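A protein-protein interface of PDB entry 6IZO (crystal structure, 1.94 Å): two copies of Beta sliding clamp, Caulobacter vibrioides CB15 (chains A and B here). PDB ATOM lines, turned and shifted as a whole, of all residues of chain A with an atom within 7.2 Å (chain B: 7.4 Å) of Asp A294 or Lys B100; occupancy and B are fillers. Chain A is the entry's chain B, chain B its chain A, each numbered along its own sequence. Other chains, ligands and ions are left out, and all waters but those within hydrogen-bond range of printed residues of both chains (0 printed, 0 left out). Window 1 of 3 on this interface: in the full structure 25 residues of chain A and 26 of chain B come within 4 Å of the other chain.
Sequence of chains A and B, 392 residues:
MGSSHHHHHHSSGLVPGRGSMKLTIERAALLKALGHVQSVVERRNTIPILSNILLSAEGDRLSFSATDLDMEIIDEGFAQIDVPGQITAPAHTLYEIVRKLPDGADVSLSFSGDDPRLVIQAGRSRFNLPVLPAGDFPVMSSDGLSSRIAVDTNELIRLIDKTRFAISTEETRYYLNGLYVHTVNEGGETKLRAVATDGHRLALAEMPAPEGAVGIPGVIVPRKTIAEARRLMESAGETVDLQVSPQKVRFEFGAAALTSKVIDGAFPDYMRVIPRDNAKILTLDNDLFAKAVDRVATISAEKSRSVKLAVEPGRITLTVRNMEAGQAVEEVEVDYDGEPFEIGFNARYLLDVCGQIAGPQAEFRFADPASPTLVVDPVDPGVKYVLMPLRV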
ATOM      1  N   LEU A 288     -25.823  15.457  23.343  1.00  0.00           N
ATOM      2  CA  LEU A 288     -24.684  16.111  22.688  1.00  0.00           C
ATOM      3  C   LEU A 288     -23.588  16.443  23.732  1.00  0.00           C
ATOM      4  O   LEU A 288     -22.427  16.121  23.540  1.00  0.00           O
ATOM      5  CB  LEU A 288     -25.126  17.388  21.973  1.00  0.00           C
ATOM      6  CG  LEU A 288     -24.026  18.396  21.572  1.00  0.00           C
ATOM      7  CD1 LEU A 288     -23.007  17.782  20.604  1.00  0.00           C
ATOM      8  CD2 LEU A 288     -24.624  19.687  21.011  1.00  0.00           C
ATOM      9  N   PHE A 289     -23.995  17.067  24.828  1.00  0.00           N
ATOM     10  CA  PHE A 289     -23.078  17.396  25.929  1.00  0.00           C
ATOM     11  C   PHE A 289     -22.349  16.166  26.479  1.00  0.00           C
ATOM     12  O   PHE A 289     -21.122  16.162  26.559  1.00  0.00           O
ATOM     13  CB  PHE A 289     -23.831  18.129  27.029  1.00  0.00           C
ATOM     14  CG  PHE A 289     -22.954  18.557  28.181  1.00  0.00           C
ATOM     15  CD1 PHE A 289     -22.043  19.587  28.016  1.00  0.00           C
ATOM     16  CD2 PHE A 289     -23.060  17.943  29.424  1.00  0.00           C
ATOM     17  CE1 PHE A 289     -21.254  20.012  29.078  1.00  0.00           C
ATOM     18  CE2 PHE A 289     -22.267  18.372  30.485  1.00  0.00           C
ATOM     19  CZ  PHE A 289     -21.363  19.395  30.304  1.00  0.00           C
ATOM     20  N   ALA A 290     -23.090  15.111  26.803  1.00  0.00           N
ATOM     21  CA  ALA A 290     -22.509  13.857  27.294  1.00  0.00           C
ATOM     22  C   ALA A 290     -21.496  13.243  26.325  1.00  0.00           C
ATOM     23  O   ALA A 290     -20.420  12.779  26.731  1.00  0.00           O
ATOM     24  CB  ALA A 290     -23.587  12.854  27.655  1.00  0.00           C
ATOM     25  N   LYS A 291     -21.814  13.295  25.038  1.00  0.00           N
ATOM     26  CA  LYS A 291     -20.887  12.795  24.031  1.00  0.00           C
ATOM     27  C   LYS A 291     -19.636  13.659  23.946  1.00  0.00           C
ATOM     28  O   LYS A 291     -18.515  13.127  23.802  1.00  0.00           O
ATOM     29  CB  LYS A 291     -21.582  12.657  22.666  1.00  0.00           C
ATOM     30  CG  LYS A 291     -22.354  11.356  22.570  1.00  0.00           C
ATOM     31  CD  LYS A 291     -23.232  11.324  21.338  1.00  0.00           C
ATOM     32  CE  LYS A 291     -24.028  10.028  21.281  1.00  0.00           C
ATOM     33  NZ  LYS A 291     -25.199  10.219  20.382  1.00  0.00           N
ATOM     34  N   ALA A 292     -19.807  14.976  24.093  1.00  0.00           N
ATOM     35  CA  ALA A 292     -18.643  15.889  24.106  1.00  0.00           C
ATOM     36  C   ALA A 292     -17.754  15.642  25.324  1.00  0.00           C
ATOM     37  O   ALA A 292     -16.526  15.578  25.195  1.00  0.00           O
ATOM     38  CB  ALA A 292     -19.071  17.339  24.009  1.00  0.00           C
ATOM     39  N   VAL A 293     -18.371  15.490  26.498  1.00  0.00           N
ATOM     40  CA  VAL A 293     -17.628  15.134  27.737  1.00  0.00           C
ATOM     41  C   VAL A 293     -16.829  13.814  27.564  1.00  0.00           C
ATOM     42  O   VAL A 293     -15.610  13.730  27.851  1.00  0.00           O
ATOM     43  CB  VAL A 293     -18.555  15.061  28.963  1.00  0.00           C
ATOM     44  CG1 VAL A 293     -17.827  14.533  30.205  1.00  0.00           C
ATOM     45  CG2 VAL A 293     -19.138  16.433  29.285  1.00  0.00           C
ATOM     46  N   ASP A 294     -17.514  12.782  27.088  1.00  0.00           N
ATOM     47  CA  ASP A 294     -16.906  11.471  26.873  1.00  0.00           C
ATOM     48  C   ASP A 294     -15.716  11.545  25.883  1.00  0.00           C
ATOM     49  O   ASP A 294     -14.642  10.950  26.103  1.00  0.00           O
ATOM     50  CB  ASP A 294     -18.002  10.498  26.415  1.00  0.00           C
ATOM     51  CG  ASP A 294     -17.503   9.093  26.232  1.00  0.00           C
ATOM     52  OD1 ASP A 294     -16.973   8.506  27.178  1.00  0.00           O
ATOM     53  OD2 ASP A 294     -17.644   8.579  25.120  1.00  0.00           O
ATOM     54  N   ARG A 295     -15.903  12.332  24.835  1.00  0.00           N
ATOM     55  CA  ARG A 295     -14.876  12.594  23.826  1.00  0.00           C
ATOM     56  C   ARG A 295     -13.628  13.249  24.415  1.00  0.00           C
ATOM     57  O   ARG A 295     -12.517  12.723  24.259  1.00  0.00           O
ATOM     58  CB  ARG A 295     -15.489  13.465  22.737  1.00  0.00           C
ATOM     59  CG  ARG A 295     -14.754  13.575  21.434  1.00  0.00           C
ATOM     60  CD  ARG A 295     -15.745  13.567  20.271  1.00  0.00           C
ATOM     61  NE  ARG A 295     -16.826  14.548  20.435  1.00  0.00           N
ATOM     62  CZ  ARG A 295     -18.118  14.345  20.167  1.00  0.00           C
ATOM     63  NH1 ARG A 295     -18.561  13.156  19.749  1.00  0.00           N
ATOM     64  NH2 ARG A 295     -18.991  15.336  20.358  1.00  0.00           N
ATOM     65  N   VAL A 296     -13.795  14.358  25.145  1.00  0.00           N
ATOM     66  CA  VAL A 296     -12.620  15.044  25.679  1.00  0.00           C
ATOM     67  C   VAL A 296     -11.942  14.237  26.780  1.00  0.00           C
ATOM     68  O   VAL A 296     -10.723  14.268  26.891  1.00  0.00           O
ATOM     69  CB  VAL A 296     -12.875  16.498  26.128  1.00  0.00           C
ATOM     70  CG1 VAL A 296     -13.287  17.339  24.942  1.00  0.00           C
ATOM     71  CG2 VAL A 296     -13.886  16.577  27.271  1.00  0.00           C
ATOM     72  N   ALA A 297     -12.716  13.482  27.551  1.00  0.00           N
ATOM     73  CA  ALA A 297     -12.173  12.623  28.615  1.00  0.00           C
ATOM     74  C   ALA A 297     -11.270  11.477  28.080  1.00  0.00           C
ATOM     75  O   ALA A 297     -10.415  10.949  28.797  1.00  0.00           O
ATOM     76  CB  ALA A 297     -13.303  12.051  29.446  1.00  0.00           C
ATOM     77  N   THR A 298     -11.453  11.116  26.820  1.00  0.00           N
ATOM     78  CA  THR A 298     -10.666  10.057  26.191  1.00  0.00           C
ATOM     79  C   THR A 298      -9.153  10.299  26.157  1.00  0.00           C
ATOM     80  O   THR A 298      -8.379   9.339  26.182  1.00  0.00           O
ATOM     81  CB  THR A 298     -11.172   9.823  24.767  1.00  0.00           C
ATOM     82  OG1 THR A 298     -12.554   9.485  24.852  1.00  0.00           O
ATOM     83  CG2 THR A 298     -10.456   8.657  24.108  1.00  0.00           C
ATOM     84  N   ILE A 299      -8.744  11.564  26.148  1.00  0.00           N
ATOM     85  CA  ILE A 299      -7.326  11.940  26.211  1.00  0.00           C
ATOM     86  C   ILE A 299      -6.600  11.325  27.403  1.00  0.00           C
ATOM     87  O   ILE A 299      -5.389  11.173  27.359  1.00  0.00           O
ATOM     88  CB  ILE A 299      -7.157  13.481  26.252  1.00  0.00           C
ATOM     89  CG1 ILE A 299      -5.750  13.901  25.824  1.00  0.00           C
ATOM     90  CG2 ILE A 299      -7.497  14.057  27.624  1.00  0.00           C
ATOM     91  CD1 ILE A 299      -5.562  13.907  24.332  1.00  0.00           C
ATOM     92  N   ARG A 305     -10.606  11.325  36.079  1.00  0.00           N
ATOM     93  CA  ARG A 305     -10.291  12.310  35.043  1.00  0.00           C
ATOM     94  C   ARG A 305     -11.157  13.520  35.365  1.00  0.00           C
ATOM     95  O   ARG A 305     -12.354  13.357  35.566  1.00  0.00           O
ATOM     96  CB  ARG A 305     -10.649  11.769  33.649  1.00  0.00           C
ATOM     97  CG  ARG A 305     -10.287  10.309  33.397  1.00  0.00           C
ATOM     98  CD  ARG A 305     -10.645   9.842  31.997  1.00  0.00           C
ATOM     99  NE  ARG A 305     -12.037   9.394  31.892  1.00  0.00           N
ATOM    100  CZ  ARG A 305     -12.559   8.728  30.856  1.00  0.00           C
ATOM    101  NH1 ARG A 305     -11.818   8.404  29.794  1.00  0.00           N
ATOM    102  NH2 ARG A 305     -13.846   8.381  30.877  1.00  0.00           N
ATOM    103  N   LEU A 318     -15.195  22.686  26.995  1.00  0.00           N
ATOM    104  CA  LEU A 318     -14.777  21.584  27.845  1.00  0.00           C
ATOM    105  C   LEU A 318     -13.304  21.318  27.611  1.00  0.00           C
ATOM    106  O   LEU A 318     -12.881  21.263  26.462  1.00  0.00           O
ATOM    107  CB  LEU A 318     -15.577  20.321  27.510  1.00  0.00           C
ATOM    108  CG  LEU A 318     -17.076  20.389  27.736  1.00  0.00           C
ATOM    109  CD1 LEU A 318     -17.756  19.253  26.974  1.00  0.00           C
ATOM    110  CD2 LEU A 318     -17.417  20.325  29.213  1.00  0.00           C
ATOM    111  N   GLU A 330     -13.294  20.888  23.521  1.00  0.00           N
ATOM    112  CA  GLU A 330     -14.489  20.917  22.668  1.00  0.00           C
ATOM    113  C   GLU A 330     -15.481  21.959  23.168  1.00  0.00           C
ATOM    114  O   GLU A 330     -15.701  22.089  24.379  1.00  0.00           O
ATOM    115  CB  GLU A 330     -15.142  19.544  22.596  1.00  0.00           C
ATOM    116  CG  GLU A 330     -16.398  19.519  21.715  1.00  0.00           C
ATOM    117  CD  GLU A 330     -16.855  18.132  21.301  1.00  0.00           C
ATOM    118  OE1 GLU A 330     -16.136  17.134  21.532  1.00  0.00           O
ATOM    119  OE2 GLU A 330     -17.960  18.038  20.707  1.00  0.00           O
ATOM    120  N   ALA A 347     -15.121  13.682  35.445  1.00  0.00           N
ATOM    121  CA  ALA A 347     -15.848  13.449  34.189  1.00  0.00           C
ATOM    122  C   ALA A 347     -16.813  12.251  34.307  1.00  0.00           C
ATOM    123  O   ALA A 347     -17.917  12.263  33.737  1.00  0.00           O
ATOM    124  CB  ALA A 347     -14.883  13.273  33.045  1.00  0.00           C
ATOM    125  N   LEU A 351     -20.811  12.280  33.746  1.00  0.00           N
ATOM    126  CA  LEU A 351     -21.416  11.314  32.823  1.00  0.00           C
ATOM    127  C   LEU A 351     -22.443  10.418  33.515  1.00  0.00           C
ATOM    128  O   LEU A 351     -23.470  10.099  32.940  1.00  0.00           O
ATOM    129  CB  LEU A 351     -20.355  10.481  32.103  1.00  0.00           C
ATOM    130  CG  LEU A 351     -19.448  11.243  31.120  1.00  0.00           C
ATOM    131  CD1 LEU A 351     -18.281  10.372  30.720  1.00  0.00           C
ATOM    132  CD2 LEU A 351     -20.190  11.710  29.870  1.00  0.00           C
ATOM    133  N   ARG B  27     -12.987   9.807   8.870  1.00  0.00           N
ATOM    134  CA  ARG B  27     -13.003   9.046  10.116  1.00  0.00           C
ATOM    135  C   ARG B  27     -13.044   7.536   9.876  1.00  0.00           C
ATOM    136  O   ARG B  27     -12.289   6.786  10.519  1.00  0.00           O
ATOM    137  CB  ARG B  27     -14.158   9.471  11.040  1.00  0.00           C
ATOM    138  CG  ARG B  27     -14.356   8.568  12.239  1.00  0.00           C
ATOM    139  CD  ARG B  27     -15.633   8.881  12.980  1.00  0.00           C
ATOM    140  NE  ARG B  27     -15.841   7.922  14.068  1.00  0.00           N
ATOM    141  CZ  ARG B  27     -16.496   6.760  13.984  1.00  0.00           C
ATOM    142  NH1 ARG B  27     -17.054   6.340  12.850  1.00  0.00           N
ATOM    143  NH2 ARG B  27     -16.605   6.005  15.070  1.00  0.00           N
ATOM    144  N   LEU B  31     -10.214   5.152  11.368  1.00  0.00           N
ATOM    145  CA  LEU B  31     -10.621   4.155  12.337  1.00  0.00           C
ATOM    146  C   LEU B  31     -10.289   2.724  11.905  1.00  0.00           C
ATOM    147  O   LEU B  31      -9.777   1.947  12.711  1.00  0.00           O
ATOM    148  CB  LEU B  31     -12.115   4.281  12.624  1.00  0.00           C
ATOM    149  CG  LEU B  31     -12.716   3.489  13.781  1.00  0.00           C
ATOM    150  CD1 LEU B  31     -12.049   3.853  15.101  1.00  0.00           C
ATOM    151  CD2 LEU B  31     -14.198   3.795  13.870  1.00  0.00           C
ATOM    152  N   LEU B  94      -5.112   7.383  20.450  1.00  0.00           N
ATOM    153  CA  LEU B  94      -5.491   7.860  19.136  1.00  0.00           C
ATOM    154  C   LEU B  94      -6.690   7.061  18.635  1.00  0.00           C
ATOM    155  O   LEU B  94      -7.637   7.640  18.108  1.00  0.00           O
ATOM    156  CB  LEU B  94      -4.300   7.807  18.153  1.00  0.00           C
ATOM    157  CG  LEU B  94      -4.555   8.394  16.764  1.00  0.00           C
ATOM    158  CD1 LEU B  94      -5.077   9.830  16.800  1.00  0.00           C
ATOM    159  CD2 LEU B  94      -3.258   8.319  15.966  1.00  0.00           C
ATOM    160  N   TYR B  95      -6.656   5.740  18.818  1.00  0.00           N
ATOM    161  CA  TYR B  95      -7.763   4.882  18.406  1.00  0.00           C
ATOM    162  C   TYR B  95      -9.071   5.289  19.114  1.00  0.00           C
ATOM    163  O   TYR B  95     -10.093   5.491  18.445  1.00  0.00           O
ATOM    164  CB  TYR B  95      -7.424   3.409  18.646  1.00  0.00           C
ATOM    165  CG  TYR B  95      -8.588   2.470  18.416  1.00  0.00           C
ATOM    166  CD1 TYR B  95      -9.080   2.230  17.133  1.00  0.00           C
ATOM    167  CD2 TYR B  95      -9.215   1.839  19.494  1.00  0.00           C
ATOM    168  CE1 TYR B  95     -10.165   1.375  16.926  1.00  0.00           C
ATOM    169  CE2 TYR B  95     -10.291   0.976  19.304  1.00  0.00           C
ATOM    170  CZ  TYR B  95     -10.762   0.751  18.020  1.00  0.00           C
ATOM    171  OH  TYR B  95     -11.825  -0.091  17.860  1.00  0.00           O
ATOM    172  N   GLU B  96      -9.015   5.454  20.435  1.00  0.00           N
ATOM    173  CA  GLU B  96     -10.197   5.780  21.238  1.00  0.00           C
ATOM    174  C   GLU B  96     -10.801   7.153  20.892  1.00  0.00           C
ATOM    175  O   GLU B  96     -12.012   7.300  20.833  1.00  0.00           O
ATOM    176  CB  GLU B  96      -9.904   5.660  22.743  1.00  0.00           C
ATOM    177  CG  GLU B  96      -9.698   4.231  23.262  1.00  0.00           C
ATOM    178  CD  GLU B  96     -10.883   3.299  22.995  1.00  0.00           C
ATOM    179  OE1 GLU B  96     -10.676   2.073  22.794  1.00  0.00           O
ATOM    180  OE2 GLU B  96     -12.024   3.792  22.970  1.00  0.00           O
ATOM    181  N   ILE B  97      -9.946   8.145  20.662  1.00  0.00           N
ATOM    182  CA  ILE B  97     -10.386   9.461  20.238  1.00  0.00           C
ATOM    183  C   ILE B  97     -11.178   9.337  18.929  1.00  0.00           C
ATOM    184  O   ILE B  97     -12.291   9.857  18.815  1.00  0.00           O
ATOM    185  CB  ILE B  97      -9.198  10.429  20.042  1.00  0.00           C
ATOM    186  CG1 ILE B  97      -8.630  10.867  21.406  1.00  0.00           C
ATOM    187  CG2 ILE B  97      -9.621  11.640  19.223  1.00  0.00           C
ATOM    188  CD1 ILE B  97      -7.283  11.569  21.329  1.00  0.00           C
ATOM    189  N   VAL B  98     -10.585   8.666  17.948  1.00  0.00           N
ATOM    190  CA  VAL B  98     -11.210   8.566  16.638  1.00  0.00           C
ATOM    191  C   VAL B  98     -12.515   7.776  16.739  1.00  0.00           C
ATOM    192  O   VAL B  98     -13.514   8.188  16.149  1.00  0.00           O
ATOM    193  CB  VAL B  98     -10.237   8.002  15.575  1.00  0.00           C
ATOM    194  CG1 VAL B  98     -10.932   7.785  14.252  1.00  0.00           C
ATOM    195  CG2 VAL B  98      -9.084   8.968  15.377  1.00  0.00           C
ATOM    196  N   ARG B  99     -12.520   6.705  17.516  1.00  0.00           N
ATOM    197  CA  ARG B  99     -13.735   5.913  17.730  1.00  0.00           C
ATOM    198  C   ARG B  99     -14.929   6.795  18.195  1.00  0.00           C
ATOM    199  O   ARG B  99     -16.057   6.630  17.733  1.00  0.00           O
ATOM    200  CB  ARG B  99     -13.478   4.789  18.742  1.00  0.00           C
ATOM    201  CG  ARG B  99     -14.430   3.610  18.610  1.00  0.00           C
ATOM    202  CD  ARG B  99     -14.072   2.433  19.532  1.00  0.00           C
ATOM    203  NE  ARG B  99     -13.944   2.837  20.934  1.00  0.00           N
ATOM    204  CZ  ARG B  99     -14.953   3.210  21.737  1.00  0.00           C
ATOM    205  NH1 ARG B  99     -16.222   3.250  21.308  1.00  0.00           N
ATOM    206  NH2 ARG B  99     -14.699   3.559  22.998  1.00  0.00           N
ATOM    207  N   LYS B 100     -14.658   7.764  19.059  1.00  0.00           N
ATOM    208  CA  LYS B 100     -15.699   8.638  19.606  1.00  0.00           C
ATOM    209  C   LYS B 100     -16.040   9.884  18.802  1.00  0.00           C
ATOM    210  O   LYS B 100     -16.918  10.635  19.194  1.00  0.00           O
ATOM    211  CB  LYS B 100     -15.297   9.044  21.017  1.00  0.00           C
ATOM    212  CG  LYS B 100     -15.261   7.839  21.920  1.00  0.00           C
ATOM    213  CD  LYS B 100     -15.050   8.253  23.354  1.00  0.00           C
ATOM    214  CE  LYS B 100     -15.125   7.051  24.294  1.00  0.00           C
ATOM    215  NZ  LYS B 100     -13.760   6.615  24.629  1.00  0.00           N
ATOM    216  N   LEU B 101     -15.314  10.141  17.728  1.00  0.00           N
ATOM    217  CA  LEU B 101     -15.647  11.225  16.830  1.00  0.00           C
ATOM    218  C   LEU B 101     -16.937  10.877  16.086  1.00  0.00           C
ATOM    219  O   LEU B 101     -17.182   9.694  15.808  1.00  0.00           O
ATOM    220  CB  LEU B 101     -14.517  11.471  15.834  1.00  0.00           C
ATOM    221  CG  LEU B 101     -13.190  11.984  16.384  1.00  0.00           C
ATOM    222  CD1 LEU B 101     -12.252  12.293  15.241  1.00  0.00           C
ATOM    223  CD2 LEU B 101     -13.341  13.209  17.280  1.00  0.00           C
ATOM    224  N   PRO B 102     -17.758  11.895  15.764  1.00  0.00           N
ATOM    225  CA  PRO B 102     -19.046  11.556  15.164  1.00  0.00           C
ATOM    226  C   PRO B 102     -18.902  10.902  13.782  1.00  0.00           C
ATOM    227  O   PRO B 102     -17.918  11.160  13.065  1.00  0.00           O
ATOM    228  CB  PRO B 102     -19.765  12.913  15.065  1.00  0.00           C
ATOM    229  CG  PRO B 102     -18.714  13.944  15.091  1.00  0.00           C
ATOM    230  CD  PRO B 102     -17.484  13.337  15.735  1.00  0.00           C
ATOM    231  N   ASP B 103     -19.875  10.059  13.424  1.00  0.00           N
ATOM    232  CA  ASP B 103     -19.902   9.389  12.113  1.00  0.00           C
ATOM    233  C   ASP B 103     -19.744  10.402  11.005  1.00  0.00           C
ATOM    234  O   ASP B 103     -20.352  11.460  11.060  1.00  0.00           O
ATOM    235  CB  ASP B 103     -21.232   8.646  11.872  1.00  0.00           C
ATOM    236  CG  ASP B 103     -21.346   7.362  12.659  1.00  0.00           C
ATOM    237  OD1 ASP B 103     -20.429   7.035  13.453  1.00  0.00           O
ATOM    238  OD2 ASP B 103     -22.367   6.666  12.478  1.00  0.00           O
ATOM    239  N   SER B 125     -14.064  19.584  17.974  1.00  0.00           N
ATOM    240  CA  SER B 125     -13.132  18.872  18.852  1.00  0.00           C
ATOM    241  C   SER B 125     -11.697  19.082  18.385  1.00  0.00           C
ATOM    242  O   SER B 125     -11.413  19.001  17.171  1.00  0.00           O
ATOM    243  CB  SER B 125     -13.427  17.365  18.851  1.00  0.00           C
ATOM    244  OG  SER B 125     -14.778  17.066  19.183  1.00  0.00           O
ATOM    245  N   PHE B 127      -7.703  17.815  19.772  1.00  0.00           N
ATOM    246  CA  PHE B 127      -6.861  17.035  20.669  1.00  0.00           C
ATOM    247  C   PHE B 127      -5.395  17.331  20.352  1.00  0.00           C
ATOM    248  O   PHE B 127      -5.048  17.539  19.189  1.00  0.00           O
ATOM    249  CB  PHE B 127      -7.128  15.546  20.503  1.00  0.00           C
ATOM    250  CG  PHE B 127      -8.556  15.153  20.723  1.00  0.00           C
ATOM    251  CD1 PHE B 127      -9.504  15.328  19.725  1.00  0.00           C
ATOM    252  CD2 PHE B 127      -8.966  14.626  21.937  1.00  0.00           C
ATOM    253  CE1 PHE B 127     -10.830  14.968  19.934  1.00  0.00           C
ATOM    254  CE2 PHE B 127     -10.290  14.260  22.151  1.00  0.00           C
ATOM    255  CZ  PHE B 127     -11.223  14.437  21.143  1.00  0.00           C
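NE of Arg B27 is in hydrogen-bond range of O of Leu B101, 2.8 Å away. The side-chain carboxylate (OE2) of Glu B96 is in salt-bridge range of the guanidinium group (NH2) of Arg B99. NZ of Lys B100 is in salt-bridge range of OE2 of Glu B96 (3.7 Å). The backbone carbonyl oxygen (O) of Asp A294 sits at hydrogen-bond distance from the side-chain hydroxyl (OG1) of Thr A298 (2.8 Å). The guanidinium group (NE) of Arg A295 is in salt-bridge range of the side-chain carboxylate (OE1) of Glu A330, 2.9 Å away. N of Leu A318 lies within hydrogen-bond range of O of Glu A330 (2.7 Å).
Lys B100 touches just these residues of chain A: Asp A294, Arg A295 and Thr A298. Printed residues of chain B within 4 Å of Thr A298: Glu B96 (3.3 Å), Ile B97 (3.5 Å) and Lys B100 (3.1 Å). Of the printed residues of chain A, Glu B96 touches Thr A298. Of the printed residues of chain A, Ile B97 touches Thr A298. Printed residues of chain A within 4 Å of Leu B101: Arg A295 (3.9 Å). The nearest residue of chain B that does not touch Asp A294 is Arg B99 (6.2 Å). The nearest printed residue of chain A that does not touch Glu B96 is Arg A295 (6.4 Å).
Of the 14 printed residues of chain B, 6 touch a printed residue of chain A. Hydrophobic or aromatic side chains of chain B that line the printed part of chain A: Ile B97, Leu B101 and Phe B127. Along chain B the printed residues that touch a printed residue of chain A span positions 96 to 127. Among the printed residues, 9 pairs touch across the chains.
O of Lys B100 sits at hydrogen-bond distance from NH1 of Arg A295 (3.1 Å). The side-chain hydroxyl (OG1) of Thr A298 lies within hydrogen-bond range of the side-chain amino group (NZ) of Lys B100, 3.1 Å away. The side-chain hydroxyl (OG) of Ser B125 lies within hydrogen-bond range of the guanidinium group (NE) of Arg A295 (3.5 Å). The side-chain carboxylate (OE1) of Glu A330 sits at hydrogen-bond distance from the side-chain hydroxyl (OG) of Ser B125 (2.7 Å).
No position is printed for both chains.
Among the printed residues, merely in contact across the chains: Asp A294 with Lys B100, Thr A298 with Glu B96, Arg A295 with Phe B127, Thr A298 with Ile B97 and Arg A295 with Leu B101.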
